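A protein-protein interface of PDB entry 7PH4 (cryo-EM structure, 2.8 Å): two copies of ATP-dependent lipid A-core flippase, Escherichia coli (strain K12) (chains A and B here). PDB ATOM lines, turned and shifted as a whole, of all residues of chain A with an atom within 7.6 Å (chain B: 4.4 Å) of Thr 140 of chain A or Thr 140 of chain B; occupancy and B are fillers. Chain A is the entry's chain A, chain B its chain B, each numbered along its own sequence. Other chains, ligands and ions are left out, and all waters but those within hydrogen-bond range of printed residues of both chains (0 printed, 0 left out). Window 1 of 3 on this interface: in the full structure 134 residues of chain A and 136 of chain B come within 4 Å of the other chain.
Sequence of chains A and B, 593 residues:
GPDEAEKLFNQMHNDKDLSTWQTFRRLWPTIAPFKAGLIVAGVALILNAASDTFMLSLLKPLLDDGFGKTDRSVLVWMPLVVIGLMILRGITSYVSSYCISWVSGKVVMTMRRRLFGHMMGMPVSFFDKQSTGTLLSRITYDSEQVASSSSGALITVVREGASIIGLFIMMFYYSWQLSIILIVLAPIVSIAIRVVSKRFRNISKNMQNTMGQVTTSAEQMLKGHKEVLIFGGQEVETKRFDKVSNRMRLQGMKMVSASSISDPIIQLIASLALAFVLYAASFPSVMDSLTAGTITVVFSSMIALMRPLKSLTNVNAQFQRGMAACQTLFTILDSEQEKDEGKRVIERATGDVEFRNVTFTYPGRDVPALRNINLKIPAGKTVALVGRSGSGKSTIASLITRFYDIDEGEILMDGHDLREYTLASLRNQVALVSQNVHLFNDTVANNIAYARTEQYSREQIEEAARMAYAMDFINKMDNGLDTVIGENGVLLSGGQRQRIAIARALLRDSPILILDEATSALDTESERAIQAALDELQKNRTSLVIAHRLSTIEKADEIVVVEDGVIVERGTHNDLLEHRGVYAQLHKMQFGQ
NH2 of Arg 112 of chain A touches CE of Met 211 of chain B (3.6 Å). CD1 of Leu 136 of chain B touches CD1 of Leu 136 of chain A, 3.6 Å away. CD2 of Leu 136 of chain A touches CG2 of Thr 215 of chain B (3.99 Å). Thr 140 of chain B touches Thr 140 of chain A. CG2 of Thr 140 of chain A touches CE of Met 211 of chain B, at 3.8 Å. Glu 144 of chain B touches Tyr 141 of chain A. CE1 of Tyr 141 of chain B touches CD of Glu 144 of chain A, 3.5 Å away. CE of Met 211 of chain A touches CG2 of Thr 140 of chain B (3.8 Å). Ala 218 of chain A touches Leu 136 of chain B (CB to CD2, 3.96 Å).
OG1 of Thr 140 of chain A lies within hydrogen-bond range of OG1 of Thr 215 of chain B (3.4 Å). The side-chain hydroxyl (OG1) of Thr 215 of chain A is in hydrogen-bond range of the side-chain hydroxyl (OG1) of Thr 140 of chain B (3.3 Å). The side-chain carboxylate (OE2) of Glu 144 of chain B sits close to the side-chain sulfur (SD) of Met 211 of chain A.
Of the 11 printed residues of chain B, 6 touch a printed residue of chain A. Hydrophobic or aromatic side chains of chain B within 4 Å of the printed part of chain A: Leu 136, Tyr 141 and Met 211. Hydrophobic or aromatic side chains of chain A that line the printed part of chain B: Leu 136, Tyr 141, Met 211 and Ala 218.
Thr 140 of chain A touches Met 211 of chain B, and with the chains exchanged Met 211 of chain A touches Thr 140 of chain B. Thr 140 of chain A touches Thr 215 of chain B, and with the chains exchanged Thr 215 of chain A touches Thr 140 of chain B. Tyr 141 of chain A touches Glu 144 of chain B, and with the chains exchanged Glu 144 of chain A touches Tyr 141 of chain B. Met 211 of chain A touches Glu 144 of chain B, but with the chains exchanged Glu 144 of chain A does not touch Met 211 of chain B (4.1 Å). 11 positions are printed for both chains. Of the 12 pairs that touch across the chains among the printed residues, 8 have their exchanged pair printed and touching as well.
Of chain B, only Thr 140, Met 211 and Thr 215 come within 4 Å of Thr 140 of chain A. Thr 140 of chain B touches just these residues of chain A: Thr 140 (3.8 Å), Met 211 (3.8 Å) and Thr 215 (3.3 Å). Printed residues of chain B within 4 Å of Ala 218 of chain A: Leu 136. Printed residues of chain B within 4 Å of Arg 112 of chain A: Met 211. Of the printed residues of chain A, Thr 215 of chain B touches Leu 136 (3.99 Å) and Thr 140 (3.4 Å). Ser 137 of chain B touches none of the printed residues of chain A. Thr 216 of chain A touches none of the printed residues of chain B. The nearest residue of chain A that does not touch Thr 140 of chain B is Tyr 141 of chain A (4.3 Å). The nearest printed residue of chain B that does not touch Thr 215 of chain A is Leu 136 of chain B (4.004 Å).
The side-chain carboxylate (OE1) of Glu 144 of chain A is in salt-bridge range of the guanidinium group (NH1) of Arg 112 of chain A (3.6 Å). The side-chain hydroxyl (OG1) of Thr 215 of chain B is in hydrogen-bond range of the backbone carbonyl oxygen (O) of Met 211 of chain B (2.9 Å). OG1 of Thr 140 of chain B lies close to O of Leu 136 of chain B (3.5 Å). O of Leu 136 of chain A sits close to OG1 of Thr 140 of chain A (3.5 Å). The backbone carbonyl oxygen of Met 211 of chain A sits at hydrogen-bond distance from the side-chain hydroxyl of Thr 215 of chain A.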
ATOM      1  N   ARG A 112      19.479 -15.035  33.835  1.00  0.00           N
ATOM      2  CA  ARG A 112      18.428 -14.055  33.589  1.00  0.00           C
ATOM      3  C   ARG A 112      18.221 -13.151  34.788  1.00  0.00           C
ATOM      4  O   ARG A 112      18.070 -11.935  34.639  1.00  0.00           O
ATOM      5  CB  ARG A 112      17.126 -14.758  33.247  1.00  0.00           C
ATOM      6  CG  ARG A 112      16.830 -14.843  31.793  1.00  0.00           C
ATOM      7  CD  ARG A 112      15.425 -15.296  31.600  1.00  0.00           C
ATOM      8  NE  ARG A 112      15.347 -16.678  31.161  1.00  0.00           N
ATOM      9  CZ  ARG A 112      14.985 -17.046  29.940  1.00  0.00           C
ATOM     10  NH1 ARG A 112      14.933 -18.324  29.617  1.00  0.00           N
ATOM     11  NH2 ARG A 112      14.661 -16.132  29.047  1.00  0.00           N
ATOM     12  N   LEU A 115      21.070 -10.687  35.055  1.00  0.00           N
ATOM     13  CA  LEU A 115      20.959  -9.651  34.039  1.00  0.00           C
ATOM     14  C   LEU A 115      19.904  -8.620  34.406  1.00  0.00           C
ATOM     15  O   LEU A 115      20.112  -7.416  34.227  1.00  0.00           O
ATOM     16  CB  LEU A 115      20.636 -10.302  32.706  1.00  0.00           C
ATOM     17  CG  LEU A 115      20.664  -9.458  31.456  1.00  0.00           C
ATOM     18  CD1 LEU A 115      22.057  -8.973  31.227  1.00  0.00           C
ATOM     19  CD2 LEU A 115      20.213 -10.317  30.322  1.00  0.00           C
ATOM     20  N   GLY A 133      14.606  -1.279  23.375  1.00  0.00           N
ATOM     21  CA  GLY A 133      14.601  -2.478  22.563  1.00  0.00           C
ATOM     22  C   GLY A 133      15.874  -3.288  22.679  1.00  0.00           C
ATOM     23  O   GLY A 133      15.834  -4.513  22.686  1.00  0.00           O
ATOM     24  N   THR A 134      17.018  -2.620  22.773  1.00  0.00           N
ATOM     25  CA  THR A 134      18.279  -3.344  22.869  1.00  0.00           C
ATOM     26  C   THR A 134      18.371  -4.135  24.167  1.00  0.00           C
ATOM     27  O   THR A 134      18.728  -5.319  24.165  1.00  0.00           O
ATOM     28  CB  THR A 134      19.437  -2.366  22.750  1.00  0.00           C
ATOM     29  OG1 THR A 134      19.356  -1.688  21.496  1.00  0.00           O
ATOM     30  CG2 THR A 134      20.742  -3.101  22.821  1.00  0.00           C
ATOM     31  N   LEU A 135      18.040  -3.503  25.291  1.00  0.00           N
ATOM     32  CA  LEU A 135      18.098  -4.189  26.574  1.00  0.00           C
ATOM     33  C   LEU A 135      17.024  -5.259  26.678  1.00  0.00           C
ATOM     34  O   LEU A 135      17.254  -6.342  27.236  1.00  0.00           O
ATOM     35  CB  LEU A 135      17.958  -3.175  27.698  1.00  0.00           C
ATOM     36  CG  LEU A 135      18.797  -1.918  27.524  1.00  0.00           C
ATOM     37  CD1 LEU A 135      18.378  -0.874  28.506  1.00  0.00           C
ATOM     38  CD2 LEU A 135      20.233  -2.259  27.715  1.00  0.00           C
ATOM     39  N   LEU A 136      15.843  -4.981  26.144  1.00  0.00           N
ATOM     40  CA  LEU A 136      14.803  -5.994  26.124  1.00  0.00           C
ATOM     41  C   LEU A 136      15.231  -7.193  25.308  1.00  0.00           C
ATOM     42  O   LEU A 136      14.905  -8.331  25.648  1.00  0.00           O
ATOM     43  CB  LEU A 136      13.519  -5.414  25.559  1.00  0.00           C
ATOM     44  CG  LEU A 136      12.544  -4.930  26.598  1.00  0.00           C
ATOM     45  CD1 LEU A 136      11.324  -4.494  25.878  1.00  0.00           C
ATOM     46  CD2 LEU A 136      12.249  -6.074  27.511  1.00  0.00           C
ATOM     47  N   SER A 137      15.928  -6.960  24.203  1.00  0.00           N
ATOM     48  CA  SER A 137      16.433  -8.075  23.427  1.00  0.00           C
ATOM     49  C   SER A 137      17.455  -8.864  24.223  1.00  0.00           C
ATOM     50  O   SER A 137      17.448 -10.091  24.194  1.00  0.00           O
ATOM     51  CB  SER A 137      17.032  -7.577  22.129  1.00  0.00           C
ATOM     52  OG  SER A 137      17.109  -8.640  21.214  1.00  0.00           O
ATOM     53  N   ARG A 138      18.325  -8.178  24.956  1.00  0.00           N
ATOM     54  CA  ARG A 138      19.261  -8.888  25.820  1.00  0.00           C
ATOM     55  C   ARG A 138      18.535  -9.833  26.763  1.00  0.00           C
ATOM     56  O   ARG A 138      18.968 -10.965  26.976  1.00  0.00           O
ATOM     57  CB  ARG A 138      20.098  -7.906  26.621  1.00  0.00           C
ATOM     58  CG  ARG A 138      21.491  -7.760  26.118  1.00  0.00           C
ATOM     59  CD  ARG A 138      21.514  -7.019  24.825  1.00  0.00           C
ATOM     60  NE  ARG A 138      22.868  -6.680  24.413  1.00  0.00           N
ATOM     61  CZ  ARG A 138      23.506  -7.262  23.407  1.00  0.00           C
ATOM     62  NH1 ARG A 138      22.909  -8.207  22.705  1.00  0.00           N
ATOM     63  NH2 ARG A 138      24.735  -6.891  23.098  1.00  0.00           N
ATOM     64  N   ILE A 139      17.434  -9.379  27.354  1.00  0.00           N
ATOM     65  CA  ILE A 139      16.697 -10.249  28.272  1.00  0.00           C
ATOM     66  C   ILE A 139      16.025 -11.390  27.522  1.00  0.00           C
ATOM     67  O   ILE A 139      16.119 -12.553  27.917  1.00  0.00           O
ATOM     68  CB  ILE A 139      15.678  -9.440  29.090  1.00  0.00           C
ATOM     69  CG1 ILE A 139      16.308  -8.965  30.387  1.00  0.00           C
ATOM     70  CG2 ILE A 139      14.476 -10.289  29.423  1.00  0.00           C
ATOM     71  CD1 ILE A 139      16.584 -10.082  31.342  1.00  0.00           C
ATOM     72  N   THR A 140      15.327 -11.080  26.435  1.00  0.00           N
ATOM     73  CA  THR A 140      14.473 -12.071  25.793  1.00  0.00           C
ATOM     74  C   THR A 140      15.253 -12.967  24.840  1.00  0.00           C
ATOM     75  O   THR A 140      15.400 -14.170  25.079  1.00  0.00           O
ATOM     76  CB  THR A 140      13.339 -11.355  25.060  1.00  0.00           C
ATOM     77  OG1 THR A 140      12.456 -10.769  26.016  1.00  0.00           O
ATOM     78  CG2 THR A 140      12.559 -12.313  24.212  1.00  0.00           C
ATOM     79  N   TYR A 141      15.818 -12.382  23.788  1.00  0.00           N
ATOM     80  CA  TYR A 141      16.397 -13.164  22.704  1.00  0.00           C
ATOM     81  C   TYR A 141      17.678 -13.871  23.127  1.00  0.00           C
ATOM     82  O   TYR A 141      17.837 -15.067  22.884  1.00  0.00           O
ATOM     83  CB  TYR A 141      16.650 -12.256  21.510  1.00  0.00           C
ATOM     84  CG  TYR A 141      17.343 -12.927  20.371  1.00  0.00           C
ATOM     85  CD1 TYR A 141      16.668 -13.789  19.546  1.00  0.00           C
ATOM     86  CD2 TYR A 141      18.670 -12.686  20.113  1.00  0.00           C
ATOM     87  CE1 TYR A 141      17.298 -14.398  18.508  1.00  0.00           C
ATOM     88  CE2 TYR A 141      19.306 -13.295  19.077  1.00  0.00           C
ATOM     89  CZ  TYR A 141      18.612 -14.148  18.278  1.00  0.00           C
ATOM     90  OH  TYR A 141      19.241 -14.762  17.234  1.00  0.00           O
ATOM     91  N   ASP A 142      18.608 -13.158  23.757  1.00  0.00           N
ATOM     92  CA  ASP A 142      19.884 -13.778  24.101  1.00  0.00           C
ATOM     93  C   ASP A 142      19.721 -14.861  25.158  1.00  0.00           C
ATOM     94  O   ASP A 142      20.329 -15.935  25.063  1.00  0.00           O
ATOM     95  CB  ASP A 142      20.867 -12.728  24.587  1.00  0.00           C
ATOM     96  CG  ASP A 142      21.102 -11.647  23.575  1.00  0.00           C
ATOM     97  OD1 ASP A 142      20.285 -11.502  22.654  1.00  0.00           O
ATOM     98  OD2 ASP A 142      22.110 -10.932  23.699  1.00  0.00           O
ATOM     99  N   SER A 143      18.920 -14.600  26.179  1.00  0.00           N
ATOM    100  CA  SER A 143      18.709 -15.625  27.184  1.00  0.00           C
ATOM    101  C   SER A 143      17.945 -16.811  26.623  1.00  0.00           C
ATOM    102  O   SER A 143      18.197 -17.951  27.027  1.00  0.00           O
ATOM    103  CB  SER A 143      17.998 -15.032  28.386  1.00  0.00           C
ATOM    104  OG  SER A 143      18.884 -14.197  29.105  1.00  0.00           O
ATOM    105  N   GLU A 144      17.043 -16.592  25.669  1.00  0.00           N
ATOM    106  CA  GLU A 144      16.407 -17.745  25.057  1.00  0.00           C
ATOM    107  C   GLU A 144      17.380 -18.531  24.194  1.00  0.00           C
ATOM    108  O   GLU A 144      17.261 -19.753  24.092  1.00  0.00           O
ATOM    109  CB  GLU A 144      15.198 -17.315  24.248  1.00  0.00           C
ATOM    110  CG  GLU A 144      14.261 -18.461  23.980  1.00  0.00           C
ATOM    111  CD  GLU A 144      13.723 -19.092  25.258  1.00  0.00           C
ATOM    112  OE1 GLU A 144      13.548 -18.361  26.254  1.00  0.00           O
ATOM    113  OE2 GLU A 144      13.478 -20.320  25.267  1.00  0.00           O
ATOM    114  N   GLN A 145      18.342 -17.858  23.569  1.00  0.00           N
ATOM    115  CA  GLN A 145      19.376 -18.571  22.831  1.00  0.00           C
ATOM    116  C   GLN A 145      20.184 -19.462  23.756  1.00  0.00           C
ATOM    117  O   GLN A 145      20.442 -20.628  23.445  1.00  0.00           O
ATOM    118  CB  GLN A 145      20.288 -17.587  22.111  1.00  0.00           C
ATOM    119  CG  GLN A 145      19.622 -16.857  20.988  1.00  0.00           C
ATOM    120  CD  GLN A 145      18.915 -17.787  20.046  1.00  0.00           C
ATOM    121  OE1 GLN A 145      19.534 -18.391  19.180  1.00  0.00           O
ATOM    122  NE2 GLN A 145      17.610 -17.909  20.205  1.00  0.00           N
ATOM    123  N   VAL A 146      20.587 -18.932  24.909  1.00  0.00           N
ATOM    124  CA  VAL A 146      21.316 -19.760  25.866  1.00  0.00           C
ATOM    125  C   VAL A 146      20.472 -20.948  26.288  1.00  0.00           C
ATOM    126  O   VAL A 146      20.960 -22.078  26.362  1.00  0.00           O
ATOM    127  CB  VAL A 146      21.750 -18.941  27.087  1.00  0.00           C
ATOM    128  CG1 VAL A 146      22.527 -19.810  28.019  1.00  0.00           C
ATOM    129  CG2 VAL A 146      22.577 -17.791  26.671  1.00  0.00           C
ATOM    130  N   MET A 211      18.915  -8.402  16.106  1.00  0.00           N
ATOM    131  CA  MET A 211      17.676  -8.635  16.832  1.00  0.00           C
ATOM    132  C   MET A 211      17.374  -7.497  17.787  1.00  0.00           C
ATOM    133  O   MET A 211      16.210  -7.154  18.007  1.00  0.00           O
ATOM    134  CB  MET A 211      17.744  -9.948  17.585  1.00  0.00           C
ATOM    135  CG  MET A 211      16.392 -10.500  17.892  1.00  0.00           C
ATOM    136  SD  MET A 211      15.495 -10.836  16.383  1.00  0.00           S
ATOM    137  CE  MET A 211      13.873 -11.121  17.044  1.00  0.00           C
ATOM    138  N   GLY A 212      18.404  -6.905  18.378  1.00  0.00           N
ATOM    139  CA  GLY A 212      18.185  -5.689  19.138  1.00  0.00           C
ATOM    140  C   GLY A 212      17.581  -4.592  18.290  1.00  0.00           C
ATOM    141  O   GLY A 212      16.687  -3.871  18.728  1.00  0.00           O
ATOM    142  N   VAL A 214      15.718  -5.026  15.581  1.00  0.00           N
ATOM    143  CA  VAL A 214      14.343  -5.413  15.279  1.00  0.00           C
ATOM    144  C   VAL A 214      13.426  -5.069  16.444  1.00  0.00           C
ATOM    145  O   VAL A 214      12.326  -4.533  16.264  1.00  0.00           O
ATOM    146  CB  VAL A 214      14.278  -6.910  14.942  1.00  0.00           C
ATOM    147  CG1 VAL A 214      12.856  -7.382  14.910  1.00  0.00           C
ATOM    148  CG2 VAL A 214      14.945  -7.175  13.628  1.00  0.00           C
ATOM    149  N   THR A 215      13.859  -5.391  17.661  1.00  0.00           N
ATOM    150  CA  THR A 215      13.053  -5.085  18.832  1.00  0.00           C
ATOM    151  C   THR A 215      12.880  -3.589  19.000  1.00  0.00           C
ATOM    152  O   THR A 215      11.798  -3.126  19.360  1.00  0.00           O
ATOM    153  CB  THR A 215      13.687  -5.683  20.074  1.00  0.00           C
ATOM    154  OG1 THR A 215      13.996  -7.050  19.822  1.00  0.00           O
ATOM    155  CG2 THR A 215      12.736  -5.615  21.223  1.00  0.00           C
ATOM    156  N   THR A 216      13.935  -2.817  18.760  1.00  0.00           N
ATOM    157  CA  THR A 216      13.812  -1.370  18.858  1.00  0.00           C
ATOM    158  C   THR A 216      12.818  -0.830  17.847  1.00  0.00           C
ATOM    159  O   THR A 216      12.012   0.043  18.169  1.00  0.00           O
ATOM    160  CB  THR A 216      15.170  -0.718  18.665  1.00  0.00           C
ATOM    161  OG1 THR A 216      15.936  -0.879  19.855  1.00  0.00           O
ATOM    162  CG2 THR A 216      15.014   0.740  18.382  1.00  0.00           C
ATOM    163  N   ALA A 218      10.190  -2.397  16.424  1.00  0.00           N
ATOM    164  CA  ALA A 218       8.827  -2.736  16.813  1.00  0.00           C
ATOM    165  C   ALA A 218       8.383  -1.948  18.035  1.00  0.00           C
ATOM    166  O   ALA A 218       7.239  -1.491  18.108  1.00  0.00           O
ATOM    167  CB  ALA A 218       8.709  -4.230  17.072  1.00  0.00           C
ATOM    168  N   LEU B 136       5.454  -7.207  21.990  1.00  0.00           N
ATOM    169  CA  LEU B 136       6.871  -7.310  21.690  1.00  0.00           C
ATOM    170  C   LEU B 136       7.333  -8.750  21.733  1.00  0.00           C
ATOM    171  O   LEU B 136       8.182  -9.159  20.942  1.00  0.00           O
ATOM    172  CB  LEU B 136       7.675  -6.479  22.672  1.00  0.00           C
ATOM    173  CG  LEU B 136       8.025  -5.099  22.183  1.00  0.00           C
ATOM    174  CD1 LEU B 136       8.884  -4.477  23.217  1.00  0.00           C
ATOM    175  CD2 LEU B 136       8.762  -5.250  20.893  1.00  0.00           C
ATOM    176  N   SER B 137       6.814  -9.528  22.675  1.00  0.00           N
ATOM    177  CA  SER B 137       7.158 -10.933  22.711  1.00  0.00           C
ATOM    178  C   SER B 137       6.646 -11.644  21.474  1.00  0.00           C
ATOM    179  O   SER B 137       7.349 -12.473  20.901  1.00  0.00           O
ATOM    180  CB  SER B 137       6.602 -11.574  23.966  1.00  0.00           C
ATOM    181  OG  SER B 137       7.286 -12.774  24.219  1.00  0.00           O
ATOM    182  N   ARG B 138       5.437 -11.317  21.033  1.00  0.00           N
ATOM    183  CA  ARG B 138       4.941 -11.893  19.789  1.00  0.00           C
ATOM    184  C   ARG B 138       5.908 -11.652  18.643  1.00  0.00           C
ATOM    185  O   ARG B 138       6.161 -12.548  17.836  1.00  0.00           O
ATOM    186  CB  ARG B 138       3.579 -11.315  19.441  1.00  0.00           C
ATOM    187  CG  ARG B 138       2.448 -12.246  19.707  1.00  0.00           C
ATOM    188  CD  ARG B 138       2.221 -12.398  21.173  1.00  0.00           C
ATOM    189  NE  ARG B 138       1.000 -13.133  21.463  1.00  0.00           N
ATOM    190  CZ  ARG B 138       0.974 -14.372  21.934  1.00  0.00           C
ATOM    191  NH1 ARG B 138       2.102 -15.011  22.177  1.00  0.00           N
ATOM    192  NH2 ARG B 138      -0.181 -14.967  22.172  1.00  0.00           N
ATOM    193  N   ILE B 139       6.449 -10.443  18.543  1.00  0.00           N
ATOM    194  CA  ILE B 139       7.387 -10.160  17.457  1.00  0.00           C
ATOM    195  C   ILE B 139       8.697 -10.911  17.657  1.00  0.00           C
ATOM    196  O   ILE B 139       9.213 -11.546  16.736  1.00  0.00           O
ATOM    197  CB  ILE B 139       7.626  -8.647  17.322  1.00  0.00           C
ATOM    198  CG1 ILE B 139       6.639  -8.050  16.336  1.00  0.00           C
ATOM    199  CG2 ILE B 139       9.025  -8.376  16.825  1.00  0.00           C
ATOM    200  CD1 ILE B 139       6.891  -8.481  14.927  1.00  0.00           C
ATOM    201  N   THR B 140       9.262 -10.844  18.856  1.00  0.00           N
ATOM    202  CA  THR B 140      10.617 -11.340  19.068  1.00  0.00           C
ATOM    203  C   THR B 140      10.643 -12.843  19.316  1.00  0.00           C
ATOM    204  O   THR B 140      11.164 -13.610  18.501  1.00  0.00           O
ATOM    205  CB  THR B 140      11.251 -10.585  20.236  1.00  0.00           C
ATOM    206  OG1 THR B 140      11.481  -9.229  19.850  1.00  0.00           O
ATOM    207  CG2 THR B 140      12.559 -11.202  20.627  1.00  0.00           C
ATOM    208  N   TYR B 141      10.026 -13.285  20.408  1.00  0.00           N
ATOM    209  CA  TYR B 141      10.172 -14.661  20.857  1.00  0.00           C
ATOM    210  C   TYR B 141       9.464 -15.645  19.935  1.00  0.00           C
ATOM    211  O   TYR B 141      10.049 -16.651  19.534  1.00  0.00           O
ATOM    212  CB  TYR B 141       9.649 -14.784  22.281  1.00  0.00           C
ATOM    213  CG  TYR B 141       9.650 -16.178  22.813  1.00  0.00           C
ATOM    214  CD1 TYR B 141      10.814 -16.779  23.214  1.00  0.00           C
ATOM    215  CD2 TYR B 141       8.479 -16.889  22.928  1.00  0.00           C
ATOM    216  CE1 TYR B 141      10.814 -18.045  23.701  1.00  0.00           C
ATOM    217  CE2 TYR B 141       8.474 -18.160  23.412  1.00  0.00           C
ATOM    218  CZ  TYR B 141       9.646 -18.730  23.798  1.00  0.00           C
ATOM    219  OH  TYR B 141       9.651 -20.003  24.288  1.00  0.00           O
ATOM    220  N   ASP B 142       8.207 -15.385  19.587  1.00  0.00           N
ATOM    221  CA  ASP B 142       7.468 -16.345  18.774  1.00  0.00           C
ATOM    222  C   ASP B 142       8.040 -16.459  17.369  1.00  0.00           C
ATOM    223  O   ASP B 142       8.168 -17.563  16.825  1.00  0.00           O
ATOM    224  CB  ASP B 142       6.001 -15.959  18.704  1.00  0.00           C
ATOM    225  CG  ASP B 142       5.365 -15.865  20.058  1.00  0.00           C
ATOM    226  OD1 ASP B 142       6.094 -15.761  21.056  1.00  0.00           O
ATOM    227  OD2 ASP B 142       4.125 -15.893  20.130  1.00  0.00           O
ATOM    228  N   SER B 143       8.378 -15.336  16.756  1.00  0.00           N
ATOM    229  CA  SER B 143       8.963 -15.407  15.430  1.00  0.00           C
ATOM    230  C   SER B 143      10.342 -16.045  15.463  1.00  0.00           C
ATOM    231  O   SER B 143      10.715 -16.749  14.518  1.00  0.00           O
ATOM    232  CB  SER B 143       9.012 -14.024  14.809  1.00  0.00           C
ATOM    233  OG  SER B 143       7.708 -13.614  14.452  1.00  0.00           O
ATOM    234  N   GLU B 144      11.102 -15.858  16.538  1.00  0.00           N
ATOM    235  CA  GLU B 144      12.366 -16.571  16.607  1.00  0.00           C
ATOM    236  C   GLU B 144      12.160 -18.065  16.800  1.00  0.00           C
ATOM    237  O   GLU B 144      12.961 -18.863  16.313  1.00  0.00           O
ATOM    238  CB  GLU B 144      13.234 -16.002  17.715  1.00  0.00           C
ATOM    239  CG  GLU B 144      13.868 -14.696  17.321  1.00  0.00           C
ATOM    240  CD  GLU B 144      14.724 -14.812  16.066  1.00  0.00           C
ATOM    241  OE1 GLU B 144      15.435 -15.827  15.923  1.00  0.00           O
ATOM    242  OE2 GLU B 144      14.688 -13.886  15.224  1.00  0.00           O
ATOM    243  N   MET B 211       6.512 -16.130  28.408  1.00  0.00           N
ATOM    244  CA  MET B 211       7.531 -15.235  27.881  1.00  0.00           C
ATOM    245  C   MET B 211       6.979 -13.838  27.668  1.00  0.00           C
ATOM    246  O   MET B 211       7.694 -12.848  27.843  1.00  0.00           O
ATOM    247  CB  MET B 211       8.093 -15.780  26.585  1.00  0.00           C
ATOM    248  CG  MET B 211       9.451 -15.238  26.281  1.00  0.00           C
ATOM    249  SD  MET B 211      10.609 -15.698  27.561  1.00  0.00           S
ATOM    250  CE  MET B 211      11.978 -14.654  27.128  1.00  0.00           C
ATOM    251  N   THR B 215       8.661 -10.522  29.395  1.00  0.00           N
ATOM    252  CA  THR B 215       8.952  -9.291  28.675  1.00  0.00           C
ATOM    253  C   THR B 215       8.223  -8.114  29.289  1.00  0.00           C
ATOM    254  O   THR B 215       8.780  -7.022  29.390  1.00  0.00           O
ATOM    255  CB  THR B 215       8.577  -9.438  27.213  1.00  0.00           C
ATOM    256  OG1 THR B 215       9.136 -10.646  26.711  1.00  0.00           O
ATOM    257  CG2 THR B 215       9.123  -8.296  26.422  1.00  0.00           C
